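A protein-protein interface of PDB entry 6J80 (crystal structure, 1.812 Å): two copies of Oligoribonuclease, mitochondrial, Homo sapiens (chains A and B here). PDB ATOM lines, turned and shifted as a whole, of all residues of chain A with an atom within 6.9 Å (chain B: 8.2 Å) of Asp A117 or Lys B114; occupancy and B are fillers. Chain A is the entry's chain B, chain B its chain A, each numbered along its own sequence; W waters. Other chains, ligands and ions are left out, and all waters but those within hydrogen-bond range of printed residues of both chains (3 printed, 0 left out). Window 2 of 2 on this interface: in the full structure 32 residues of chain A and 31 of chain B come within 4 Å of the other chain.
OE2 of Glu B111 lies within salt-bridge range of NZ of Lys A113.
NZ of Lys B114 is in salt-bridge range of OD2 of Asp A117 (2.7 Å).
OD2 of Asp B117 is in salt-bridge range of NZ of Lys A114.
The side-chain amino group of Lys B114 lies within salt-bridge range of the side-chain carboxylate of Glu B111 (3.8 Å).
The side-chain amino group (NZ) of Lys B113 is in salt-bridge range of the side-chain carboxylate (OD2) of Asp B117, 3.0 Å away.
NZ of Lys A113 lies within salt-bridge range of OD2 of Asp A117.
His A110 touches His B110 (CB to CB, 3.4 Å).
His A110 touches Ile B131.
Of the printed residues of chain B, Asp A117 touches Lys B114.
Lys B114 touches just one residue of chain A: Asp A117.
Of the printed residues of chain A, Asp B117 touches Lys A114 (2.8 Å).
Printed residues of chain B within 4 Å of His A110: His B110 and Ile B131.
Printed residues of chain A within 4 Å of His B110: His A110 (3.4 Å).
Of the printed residues of chain A, Glu B111 touches Lys A113.
Printed residues of chain A within 4 Å of Ile B131: His A110.
The nearest residue of chain A that does not touch Lys B114 is Lys A113 (4.3 Å).
Of the 17 printed residues of chain B, 5 touch a printed residue of chain A.
Hydrophobic or aromatic side chains of chain B within 4 Å of the printed part of chain A: His B110 and Ile B131.
Of the 16 printed residues of chain A, 4 touch a printed residue of chain B.
Among the printed residues, 5 pairs touch across the chains.
Among the printed residues, Asp or Glu carboxylates within 4 Å of a Lys or Arg side-chain nitrogen of the other chain: Lys A113 with Glu B111 (3.1 Å), Lys A114 with Asp B117 (2.8 Å) and Asp A117 with Lys B114 (2.7 Å).
His B110 touches its own counterpart, His A110.
Lys A114 touches Asp B117, and with the chains exchanged Asp A117 touches Lys B114.
Positions printed for both chains: 104, 110, 112, 113, 114, 115, 116, 117, 118, 119, 120 and 124.
Water W2 lies within hydrogen-bond range of the side-chain carboxylate (OE2) of Glu B111, a ring nitrogen (ND1) of His B110 and the side-chain amino group (NZ) of Lys A113.
Water W3 bridges a ring nitrogen (ND1) of His A110 and the side-chain amino group of Lys B113.
Water W1 bridges the backbone NH (N) of Ile B131 and a ring nitrogen (NE2) of His A110.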
ATOM      1  N   ILE A  20      -0.795  29.681  28.253  1.00  0.00           N
ATOM      2  CA  ILE A  20      -0.478  30.374  27.009  1.00  0.00           C
ATOM      3  C   ILE A  20      -0.140  31.839  27.248  1.00  0.00           C
ATOM      4  O   ILE A  20       0.532  32.465  26.420  1.00  0.00           O
ATOM      5  CB  ILE A  20      -1.651  30.234  26.017  1.00  0.00           C
ATOM      6  CG1 ILE A  20      -1.265  30.763  24.633  1.00  0.00           C
ATOM      7  CG2 ILE A  20      -2.892  30.943  26.561  1.00  0.00           C
ATOM      8  CD1 ILE A  20      -0.028  30.109  24.033  1.00  0.00           C
ATOM      9  N   LEU A 104      -0.608  20.065  10.755  1.00  0.00           N
ATOM     10  CA  LEU A 104       0.167  19.624  11.905  1.00  0.00           C
ATOM     11  C   LEU A 104      -0.333  18.258  12.370  1.00  0.00           C
ATOM     12  O   LEU A 104      -1.538  17.996  12.377  1.00  0.00           O
ATOM     13  CB  LEU A 104       0.015  20.606  13.063  1.00  0.00           C
ATOM     14  CG  LEU A 104       0.779  21.911  13.099  1.00  0.00           C
ATOM     15  CD1 LEU A 104       0.312  22.668  14.351  1.00  0.00           C
ATOM     16  CD2 LEU A 104       2.280  21.646  13.128  1.00  0.00           C
ATOM     17  N   HIS A 110      -3.152  19.937  19.249  1.00  0.00           N
ATOM     18  CA  HIS A 110      -3.830  21.223  19.389  1.00  0.00           C
ATOM     19  C   HIS A 110      -3.160  22.108  20.435  1.00  0.00           C
ATOM     20  O   HIS A 110      -3.212  23.338  20.333  1.00  0.00           O
ATOM     21  CB  HIS A 110      -5.292  21.011  19.758  1.00  0.00           C
ATOM     22  CG  HIS A 110      -5.480  20.050  20.883  1.00  0.00           C
ATOM     23  ND1 HIS A 110      -5.603  20.454  22.196  1.00  0.00           N
ATOM     24  CD2 HIS A 110      -5.543  18.698  20.897  1.00  0.00           C
ATOM     25  CE1 HIS A 110      -5.748  19.393  22.969  1.00  0.00           C
ATOM     26  NE2 HIS A 110      -5.705  18.315  22.204  1.00  0.00           N
ATOM     27  N   ASP A 112       0.210  22.223  21.080  1.00  0.00           N
ATOM     28  CA  ASP A 112       1.324  22.800  20.338  1.00  0.00           C
ATOM     29  C   ASP A 112       0.834  23.853  19.363  1.00  0.00           C
ATOM     30  O   ASP A 112       1.500  24.873  19.168  1.00  0.00           O
ATOM     31  CB  ASP A 112       2.091  21.724  19.573  1.00  0.00           C
ATOM     32  CG  ASP A 112       2.359  20.489  20.404  1.00  0.00           C
ATOM     33  OD1 ASP A 112       1.402  19.718  20.675  1.00  0.00           O
ATOM     34  OD2 ASP A 112       3.536  20.267  20.762  1.00  0.00           O
ATOM     35  N   LYS A 113      -0.313  23.614  18.725  1.00  0.00           N
ATOM     36  CA  LYS A 113      -0.824  24.594  17.767  1.00  0.00           C
ATOM     37  C   LYS A 113      -1.189  25.898  18.464  1.00  0.00           C
ATOM     38  O   LYS A 113      -0.960  26.976  17.916  1.00  0.00           O
ATOM     39  CB  LYS A 113      -2.029  24.039  17.011  1.00  0.00           C
ATOM     40  CG  LYS A 113      -2.559  24.970  15.901  1.00  0.00           C
ATOM     41  CD  LYS A 113      -3.722  24.358  15.131  1.00  0.00           C
ATOM     42  CE  LYS A 113      -4.264  25.310  14.065  1.00  0.00           C
ATOM     43  NZ  LYS A 113      -4.901  26.515  14.691  1.00  0.00           N
ATOM     44  N   LYS A 114      -1.756  25.827  19.671  1.00  0.00           N
ATOM     45  CA  LYS A 114      -2.048  27.064  20.401  1.00  0.00           C
ATOM     46  C   LYS A 114      -0.770  27.881  20.596  1.00  0.00           C
ATOM     47  O   LYS A 114      -0.719  29.101  20.308  1.00  0.00           O
ATOM     48  CB  LYS A 114      -2.712  26.716  21.741  1.00  0.00           C
ATOM     49  CG  LYS A 114      -2.936  27.879  22.692  1.00  0.00           C
ATOM     50  CD  LYS A 114      -3.277  27.374  24.091  1.00  0.00           C
ATOM     51  CE  LYS A 114      -4.495  26.471  24.061  1.00  0.00           C
ATOM     52  NZ  LYS A 114      -5.208  26.473  25.369  1.00  0.00           N
ATOM     53  N   PHE A 115       0.305  27.199  20.999  1.00  0.00           N
ATOM     54  CA  PHE A 115       1.558  27.918  21.234  1.00  0.00           C
ATOM     55  C   PHE A 115       2.188  28.417  19.937  1.00  0.00           C
ATOM     56  O   PHE A 115       2.755  29.514  19.902  1.00  0.00           O
ATOM     57  CB  PHE A 115       2.538  27.038  22.006  1.00  0.00           C
ATOM     58  CG  PHE A 115       2.316  27.074  23.492  1.00  0.00           C
ATOM     59  CD1 PHE A 115       1.324  26.302  24.074  1.00  0.00           C
ATOM     60  CD2 PHE A 115       3.071  27.912  24.301  1.00  0.00           C
ATOM     61  CE1 PHE A 115       1.105  26.339  25.448  1.00  0.00           C
ATOM     62  CE2 PHE A 115       2.855  27.966  25.681  1.00  0.00           C
ATOM     63  CZ  PHE A 115       1.874  27.177  26.254  1.00  0.00           C
ATOM     64  N   LEU A 116       2.121  27.627  18.863  1.00  0.00           N
ATOM     65  CA  LEU A 116       2.723  28.051  17.602  1.00  0.00           C
ATOM     66  C   LEU A 116       1.936  29.194  16.969  1.00  0.00           C
ATOM     67  O   LEU A 116       2.526  30.099  16.363  1.00  0.00           O
ATOM     68  CB  LEU A 116       2.807  26.873  16.629  1.00  0.00           C
ATOM     69  CG  LEU A 116       3.735  25.745  17.070  1.00  0.00           C
ATOM     70  CD1 LEU A 116       3.500  24.479  16.253  1.00  0.00           C
ATOM     71  CD2 LEU A 116       5.181  26.203  16.954  1.00  0.00           C
ATOM     72  N   ASP A 117       0.607  29.139  17.056  1.00  0.00           N
ATOM     73  CA  ASP A 117      -0.223  30.225  16.550  1.00  0.00           C
ATOM     74  C   ASP A 117       0.179  31.535  17.204  1.00  0.00           C
ATOM     75  O   ASP A 117       0.240  32.575  16.534  1.00  0.00           O
ATOM     76  CB  ASP A 117      -1.707  29.940  16.812  1.00  0.00           C
ATOM     77  CG  ASP A 117      -2.304  28.924  15.840  1.00  0.00           C
ATOM     78  OD1 ASP A 117      -1.669  28.628  14.811  1.00  0.00           O
ATOM     79  OD2 ASP A 117      -3.423  28.437  16.116  1.00  0.00           O
ATOM     80  N   LYS A 118       0.488  31.492  18.505  1.00  0.00           N
ATOM     81  CA  LYS A 118       0.938  32.709  19.188  1.00  0.00           C
ATOM     82  C   LYS A 118       2.375  33.094  18.809  1.00  0.00           C
ATOM     83  O   LYS A 118       2.647  34.248  18.447  1.00  0.00           O
ATOM     84  CB  LYS A 118       0.806  32.532  20.699  1.00  0.00           C
ATOM     85  CG  LYS A 118       1.034  33.826  21.492  1.00  0.00           C
ATOM     86  CD  LYS A 118       0.944  33.617  22.989  1.00  0.00           C
ATOM     87  CE  LYS A 118       0.966  34.957  23.726  1.00  0.00           C
ATOM     88  NZ  LYS A 118       1.122  34.801  25.200  1.00  0.00           N
ATOM     89  N   TYR A 119       3.313  32.147  18.880  1.00  0.00           N
ATOM     90  CA  TYR A 119       4.732  32.481  18.890  1.00  0.00           C
ATOM     91  C   TYR A 119       5.454  32.241  17.575  1.00  0.00           C
ATOM     92  O   TYR A 119       6.534  32.807  17.375  1.00  0.00           O
ATOM     93  CB  TYR A 119       5.445  31.703  19.995  1.00  0.00           C
ATOM     94  CG  TYR A 119       5.048  32.189  21.356  1.00  0.00           C
ATOM     95  CD1 TYR A 119       5.326  33.495  21.747  1.00  0.00           C
ATOM     96  CD2 TYR A 119       4.380  31.361  22.249  1.00  0.00           C
ATOM     97  CE1 TYR A 119       4.960  33.955  22.989  1.00  0.00           C
ATOM     98  CE2 TYR A 119       4.004  31.817  23.495  1.00  0.00           C
ATOM     99  CZ  TYR A 119       4.302  33.115  23.861  1.00  0.00           C
ATOM    100  OH  TYR A 119       3.936  33.573  25.113  1.00  0.00           O
ATOM    101  N   MET A 120       4.915  31.405  16.690  1.00  0.00           N
ATOM    102  CA  MET A 120       5.475  31.206  15.355  1.00  0.00           C
ATOM    103  C   MET A 120       4.386  31.390  14.304  1.00  0.00           C
ATOM    104  O   MET A 120       4.133  30.499  13.486  1.00  0.00           O
ATOM    105  CB  MET A 120       6.129  29.831  15.233  1.00  0.00           C
ATOM    106  CG  MET A 120       7.251  29.596  16.221  1.00  0.00           C
ATOM    107  SD  MET A 120       8.323  28.248  15.696  1.00  0.00           S
ATOM    108  CE  MET A 120       9.519  28.198  17.036  1.00  0.00           C
ATOM    109  N   PRO A 121       3.735  32.562  14.277  1.00  0.00           N
ATOM    110  CA  PRO A 121       2.609  32.744  13.341  1.00  0.00           C
ATOM    111  C   PRO A 121       2.990  32.597  11.871  1.00  0.00           C
ATOM    112  O   PRO A 121       2.156  32.141  11.075  1.00  0.00           O
ATOM    113  CB  PRO A 121       2.114  34.164  13.665  1.00  0.00           C
ATOM    114  CG  PRO A 121       3.288  34.855  14.294  1.00  0.00           C
ATOM    115  CD  PRO A 121       3.999  33.779  15.071  1.00  0.00           C
ATOM    116  N   GLN A 122       4.220  32.955  11.480  1.00  0.00           N
ATOM    117  CA  GLN A 122       4.607  32.834  10.075  1.00  0.00           C
ATOM    118  C   GLN A 122       4.759  31.375   9.674  1.00  0.00           C
ATOM    119  O   GLN A 122       4.416  30.991   8.547  1.00  0.00           O
ATOM    120  CB  GLN A 122       5.913  33.593   9.800  1.00  0.00           C
ATOM    121  CG  GLN A 122       5.903  35.101  10.137  1.00  0.00           C
ATOM    122  CD  GLN A 122       4.634  35.808   9.686  1.00  0.00           C
ATOM    123  OE1 GLN A 122       4.051  35.479   8.647  1.00  0.00           O
ATOM    124  NE2 GLN A 122       4.193  36.783  10.478  1.00  0.00           N
ATOM    125  N   MET A 124       2.992  28.961  11.066  1.00  0.00           N
ATOM    126  CA  MET A 124       1.636  28.434  10.997  1.00  0.00           C
ATOM    127  C   MET A 124       0.882  28.904   9.757  1.00  0.00           C
ATOM    128  O   MET A 124      -0.046  28.216   9.314  1.00  0.00           O
ATOM    129  CB  MET A 124       0.868  28.810  12.255  1.00  0.00           C
ATOM    130  CG  MET A 124       1.322  28.040  13.498  1.00  0.00           C
ATOM    131  SD  MET A 124       1.296  26.231  13.278  1.00  0.00           S
ATOM    132  CE  MET A 124      -0.377  25.967  12.677  1.00  0.00           C
ATOM    133  N   LYS A 125       1.256  30.055   9.185  1.00  0.00           N
ATOM    134  CA  LYS A 125       0.637  30.490   7.934  1.00  0.00           C
ATOM    135  C   LYS A 125       0.901  29.506   6.798  1.00  0.00           C
ATOM    136  O   LYS A 125       0.099  29.417   5.861  1.00  0.00           O
ATOM    137  CB  LYS A 125       1.136  31.887   7.547  1.00  0.00           C
ATOM    138  CG  LYS A 125       0.452  33.000   8.324  1.00  0.00           C
ATOM    139  CD  LYS A 125       0.691  34.362   7.695  1.00  0.00           C
ATOM    140  CE  LYS A 125       0.226  35.479   8.617  1.00  0.00           C
ATOM    141  NZ  LYS A 125       1.392  36.134   9.282  1.00  0.00           N
ATOM    142  N   LEU B  13     -19.474  26.311  18.396  1.00  0.00           N
ATOM    143  CA  LEU B  13     -19.621  27.757  18.469  1.00  0.00           C
ATOM    144  C   LEU B  13     -19.698  28.324  17.058  1.00  0.00           C
ATOM    145  O   LEU B  13     -18.925  27.927  16.188  1.00  0.00           O
ATOM    146  CB  LEU B  13     -18.440  28.389  19.198  1.00  0.00           C
ATOM    147  CG  LEU B  13     -18.440  28.372  20.722  1.00  0.00           C
ATOM    148  CD1 LEU B  13     -18.222  26.974  21.288  1.00  0.00           C
ATOM    149  CD2 LEU B  13     -17.345  29.304  21.185  1.00  0.00           C
ATOM    150  N   LEU B 104     -13.886  17.151  25.023  1.00  0.00           N
ATOM    151  CA  LEU B 104     -14.588  17.901  23.996  1.00  0.00           C
ATOM    152  C   LEU B 104     -14.567  17.135  22.688  1.00  0.00           C
ATOM    153  O   LEU B 104     -13.556  16.530  22.329  1.00  0.00           O
ATOM    154  CB  LEU B 104     -13.918  19.248  23.751  1.00  0.00           C
ATOM    155  CG  LEU B 104     -14.249  20.414  24.640  1.00  0.00           C
ATOM    156  CD1 LEU B 104     -13.511  21.646  24.080  1.00  0.00           C
ATOM    157  CD2 LEU B 104     -15.770  20.636  24.739  1.00  0.00           C
ATOM    158  N   SER B 108     -12.940  19.980  14.051  1.00  0.00           N
ATOM    159  CA  SER B 108     -11.873  20.934  14.394  1.00  0.00           C
ATOM    160  C   SER B 108     -12.141  21.601  15.749  1.00  0.00           C
ATOM    161  O   SER B 108     -11.974  22.813  15.923  1.00  0.00           O
ATOM    162  CB  SER B 108     -11.703  21.987  13.295  1.00  0.00           C
ATOM    163  OG  SER B 108     -11.059  21.419  12.167  1.00  0.00           O
ATOM    164  N   VAL B 109     -12.582  20.799  16.716  1.00  0.00           N
ATOM    165  CA  VAL B 109     -12.987  21.342  18.012  1.00  0.00           C
ATOM    166  C   VAL B 109     -11.824  21.959  18.778  1.00  0.00           C
ATOM    167  O   VAL B 109     -12.042  22.625  19.791  1.00  0.00           O
ATOM    168  CB  VAL B 109     -13.715  20.217  18.786  1.00  0.00           C
ATOM    169  CG1 VAL B 109     -12.732  19.186  19.334  1.00  0.00           C
ATOM    170  CG2 VAL B 109     -14.618  20.792  19.887  1.00  0.00           C
ATOM    171  N   HIS B 110     -10.583  21.804  18.305  1.00  0.00           N
ATOM    172  CA  HIS B 110      -9.486  22.534  18.938  1.00  0.00           C
ATOM    173  C   HIS B 110      -9.661  24.048  18.817  1.00  0.00           C
ATOM    174  O   HIS B 110      -9.208  24.799  19.690  1.00  0.00           O
ATOM    175  CB  HIS B 110      -8.148  22.122  18.332  1.00  0.00           C
ATOM    176  CG  HIS B 110      -8.117  22.191  16.841  1.00  0.00           C
ATOM    177  ND1 HIS B 110      -7.610  23.276  16.162  1.00  0.00           N
ATOM    178  CD2 HIS B 110      -8.515  21.305  15.896  1.00  0.00           C
ATOM    179  CE1 HIS B 110      -7.706  23.062  14.861  1.00  0.00           C
ATOM    180  NE2 HIS B 110      -8.258  21.877  14.672  1.00  0.00           N
ATOM    181  N   GLU B 111     -10.314  24.520  17.757  1.00  0.00           N
ATOM    182  CA  GLU B 111     -10.565  25.957  17.653  1.00  0.00           C
ATOM    183  C   GLU B 111     -11.553  26.414  18.728  1.00  0.00           C
ATOM    184  O   GLU B 111     -11.326  27.422  19.431  1.00  0.00           O
ATOM    185  CB  GLU B 111     -11.072  26.288  16.252  1.00  0.00           C
ATOM    186  CG  GLU B 111      -9.939  26.509  15.265  1.00  0.00           C
ATOM    187  CD  GLU B 111      -8.951  27.562  15.762  1.00  0.00           C
ATOM    188  OE1 GLU B 111      -9.399  28.647  16.198  1.00  0.00           O
ATOM    189  OE2 GLU B 111      -7.729  27.299  15.730  1.00  0.00           O
ATOM    190  N   ASP B 112     -12.645  25.656  18.888  1.00  0.00           N
ATOM    191  CA  ASP B 112     -13.576  25.899  19.985  1.00  0.00           C
ATOM    192  C   ASP B 112     -12.862  25.849  21.327  1.00  0.00           C
ATOM    193  O   ASP B 112     -13.110  26.687  22.204  1.00  0.00           O
ATOM    194  CB  ASP B 112     -14.705  24.859  19.972  1.00  0.00           C
ATOM    195  CG  ASP B 112     -15.432  24.788  18.645  1.00  0.00           C
ATOM    196  OD1 ASP B 112     -16.398  25.548  18.458  1.00  0.00           O
ATOM    197  OD2 ASP B 112     -15.059  23.954  17.794  1.00  0.00           O
ATOM    198  N   LYS B 113     -11.986  24.859  21.512  1.00  0.00           N
ATOM    199  CA  LYS B 113     -11.296  24.711  22.782  1.00  0.00           C
ATOM    200  C   LYS B 113     -10.393  25.902  23.069  1.00  0.00           C
ATOM    201  O   LYS B 113     -10.276  26.318  24.218  1.00  0.00           O
ATOM    202  CB  LYS B 113     -10.483  23.419  22.802  1.00  0.00           C
ATOM    203  CG  LYS B 113      -9.862  23.133  24.168  1.00  0.00           C
ATOM    204  CD  LYS B 113      -9.049  21.827  24.153  1.00  0.00           C
ATOM    205  CE  LYS B 113      -8.507  21.482  25.542  1.00  0.00           C
ATOM    206  NZ  LYS B 113      -7.231  22.196  25.852  1.00  0.00           N
ATOM    207  N   LYS B 114      -9.725  26.450  22.048  1.00  0.00           N
ATOM    208  CA  LYS B 114      -8.911  27.644  22.273  1.00  0.00           C
ATOM    209  C   LYS B 114      -9.769  28.778  22.842  1.00  0.00           C
ATOM    210  O   LYS B 114      -9.431  29.401  23.878  1.00  0.00           O
ATOM    211  CB  LYS B 114      -8.227  28.049  20.954  1.00  0.00           C
ATOM    212  CG  LYS B 114      -7.327  29.271  21.032  1.00  0.00           C
ATOM    213  CD  LYS B 114      -6.135  29.191  20.072  1.00  0.00           C
ATOM    214  CE  LYS B 114      -6.542  29.398  18.625  1.00  0.00           C
ATOM    215  NZ  LYS B 114      -5.357  29.494  17.710  1.00  0.00           N
ATOM    216  N   PHE B 115     -10.938  28.990  22.227  1.00  0.00           N
ATOM    217  CA  PHE B 115     -11.849  30.025  22.730  1.00  0.00           C
ATOM    218  C   PHE B 115     -12.328  29.719  24.155  1.00  0.00           C
ATOM    219  O   PHE B 115     -12.319  30.597  25.028  1.00  0.00           O
ATOM    220  CB  PHE B 115     -13.041  30.189  21.787  1.00  0.00           C
ATOM    221  CG  PHE B 115     -14.069  31.187  22.274  1.00  0.00           C
ATOM    222  CD1 PHE B 115     -15.075  30.799  23.153  1.00  0.00           C
ATOM    223  CD2 PHE B 115     -14.026  32.516  21.859  1.00  0.00           C
ATOM    224  CE1 PHE B 115     -16.033  31.711  23.605  1.00  0.00           C
ATOM    225  CE2 PHE B 115     -14.972  33.434  22.313  1.00  0.00           C
ATOM    226  CZ  PHE B 115     -15.972  33.028  23.186  1.00  0.00           C
ATOM    227  N   LEU B 116     -12.771  28.481  24.401  1.00  0.00           N
ATOM    228  CA  LEU B 116     -13.337  28.129  25.701  1.00  0.00           C
ATOM    229  C   LEU B 116     -12.276  28.120  26.796  1.00  0.00           C
ATOM    230  O   LEU B 116     -12.576  28.443  27.948  1.00  0.00           O
ATOM    231  CB  LEU B 116     -14.012  26.763  25.623  1.00  0.00           C
ATOM    232  CG  LEU B 116     -15.241  26.694  24.717  1.00  0.00           C
ATOM    233  CD1 LEU B 116     -15.604  25.236  24.472  1.00  0.00           C
ATOM    234  CD2 LEU B 116     -16.428  27.443  25.325  1.00  0.00           C
ATOM    235  N   ASP B 117     -11.048  27.702  26.465  1.00  0.00           N
ATOM    236  CA  ASP B 117      -9.951  27.748  27.425  1.00  0.00           C
ATOM    237  C   ASP B 117      -9.749  29.169  27.912  1.00  0.00           C
ATOM    238  O   ASP B 117      -9.482  29.394  29.098  1.00  0.00           O
ATOM    239  CB  ASP B 117      -8.648  27.240  26.794  1.00  0.00           C
ATOM    240  CG  ASP B 117      -8.545  25.707  26.762  1.00  0.00           C
ATOM    241  OD1 ASP B 117      -9.370  25.025  27.408  1.00  0.00           O
ATOM    242  OD2 ASP B 117      -7.616  25.190  26.100  1.00  0.00           O
ATOM    243  N   LYS B 118      -9.875  30.143  27.005  1.00  0.00           N
ATOM    244  CA  LYS B 118      -9.672  31.529  27.435  1.00  0.00           C
ATOM    245  C   LYS B 118     -10.898  32.122  28.137  1.00  0.00           C
ATOM    246  O   LYS B 118     -10.771  32.756  29.194  1.00  0.00           O
ATOM    247  CB  LYS B 118      -9.292  32.393  26.237  1.00  0.00           C
ATOM    248  CG  LYS B 118      -9.133  33.872  26.593  1.00  0.00           C
ATOM    249  CD  LYS B 118      -8.619  34.671  25.411  1.00  0.00           C
ATOM    250  CE  LYS B 118      -8.280  36.098  25.833  1.00  0.00           C
ATOM    251  NZ  LYS B 118      -7.325  36.736  24.884  1.00  0.00           N
ATOM    252  N   TYR B 119     -12.088  31.948  27.565  1.00  0.00           N
ATOM    253  CA  TYR B 119     -13.276  32.672  28.010  1.00  0.00           C
ATOM    254  C   TYR B 119     -14.225  31.867  28.885  1.00  0.00           C
ATOM    255  O   TYR B 119     -15.079  32.471  29.534  1.00  0.00           O
ATOM    256  CB  TYR B 119     -14.056  33.203  26.803  1.00  0.00           C
ATOM    257  CG  TYR B 119     -13.248  34.235  26.051  1.00  0.00           C
ATOM    258  CD1 TYR B 119     -13.030  35.498  26.595  1.00  0.00           C
ATOM    259  CD2 TYR B 119     -12.664  33.938  24.827  1.00  0.00           C
ATOM    260  CE1 TYR B 119     -12.277  36.440  25.932  1.00  0.00           C
ATOM    261  CE2 TYR B 119     -11.904  34.883  24.151  1.00  0.00           C
ATOM    262  CZ  TYR B 119     -11.713  36.129  24.712  1.00  0.00           C
ATOM    263  OH  TYR B 119     -10.962  37.077  24.053  1.00  0.00           O
ATOM    264  N   MET B 120     -14.117  30.537  28.916  1.00  0.00           N
ATOM    265  CA  MET B 120     -14.920  29.699  29.811  1.00  0.00           C
ATOM    266  C   MET B 120     -14.019  28.716  30.554  1.00  0.00           C
ATOM    267  O   MET B 120     -14.214  27.493  30.477  1.00  0.00           O
ATOM    268  CB  MET B 120     -16.013  28.957  29.041  1.00  0.00           C
ATOM    269  CG  MET B 120     -17.037  29.887  28.344  1.00  0.00           C
ATOM    270  SD  MET B 120     -18.590  29.050  27.993  1.00  0.00           S
ATOM    271  CE  MET B 120     -19.579  30.419  27.374  1.00  0.00           C
ATOM    272  N   MET B 124     -14.084  24.460  31.072  1.00  0.00           N
ATOM    273  CA  MET B 124     -13.018  23.580  30.590  1.00  0.00           C
ATOM    274  C   MET B 124     -12.345  22.814  31.724  1.00  0.00           C
ATOM    275  O   MET B 124     -11.820  21.725  31.495  1.00  0.00           O
ATOM    276  CB  MET B 124     -11.980  24.379  29.806  1.00  0.00           C
ATOM    277  CG  MET B 124     -12.471  24.862  28.424  1.00  0.00           C
ATOM    278  SD  MET B 124     -13.207  23.551  27.406  1.00  0.00           S
ATOM    279  CE  MET B 124     -11.894  22.326  27.419  1.00  0.00           C
ATOM    280  N   ILE B 131      -9.032  15.877  23.119  1.00  0.00           N
ATOM    281  CA  ILE B 131     -10.235  16.153  22.349  1.00  0.00           C
ATOM    282  C   ILE B 131     -10.510  14.977  21.433  1.00  0.00           C
ATOM    283  O   ILE B 131      -9.628  14.168  21.127  1.00  0.00           O
ATOM    284  CB  ILE B 131     -10.132  17.452  21.505  1.00  0.00           C
ATOM    285  CG1 ILE B 131      -8.986  17.322  20.492  1.00  0.00           C
ATOM    286  CG2 ILE B 131      -9.944  18.659  22.409  1.00  0.00           C
ATOM    287  CD1 ILE B 131      -8.784  18.564  19.614  1.00  0.00           C
HETATM  288  O   HOH W   1      -6.310  15.360  22.017  1.00  0.00           O
HETATM  289  O   HOH W   2      -6.372  25.666  16.962  1.00  0.00           O
HETATM  290  O   HOH W   3      -5.408  22.709  23.587  1.00  0.00           O
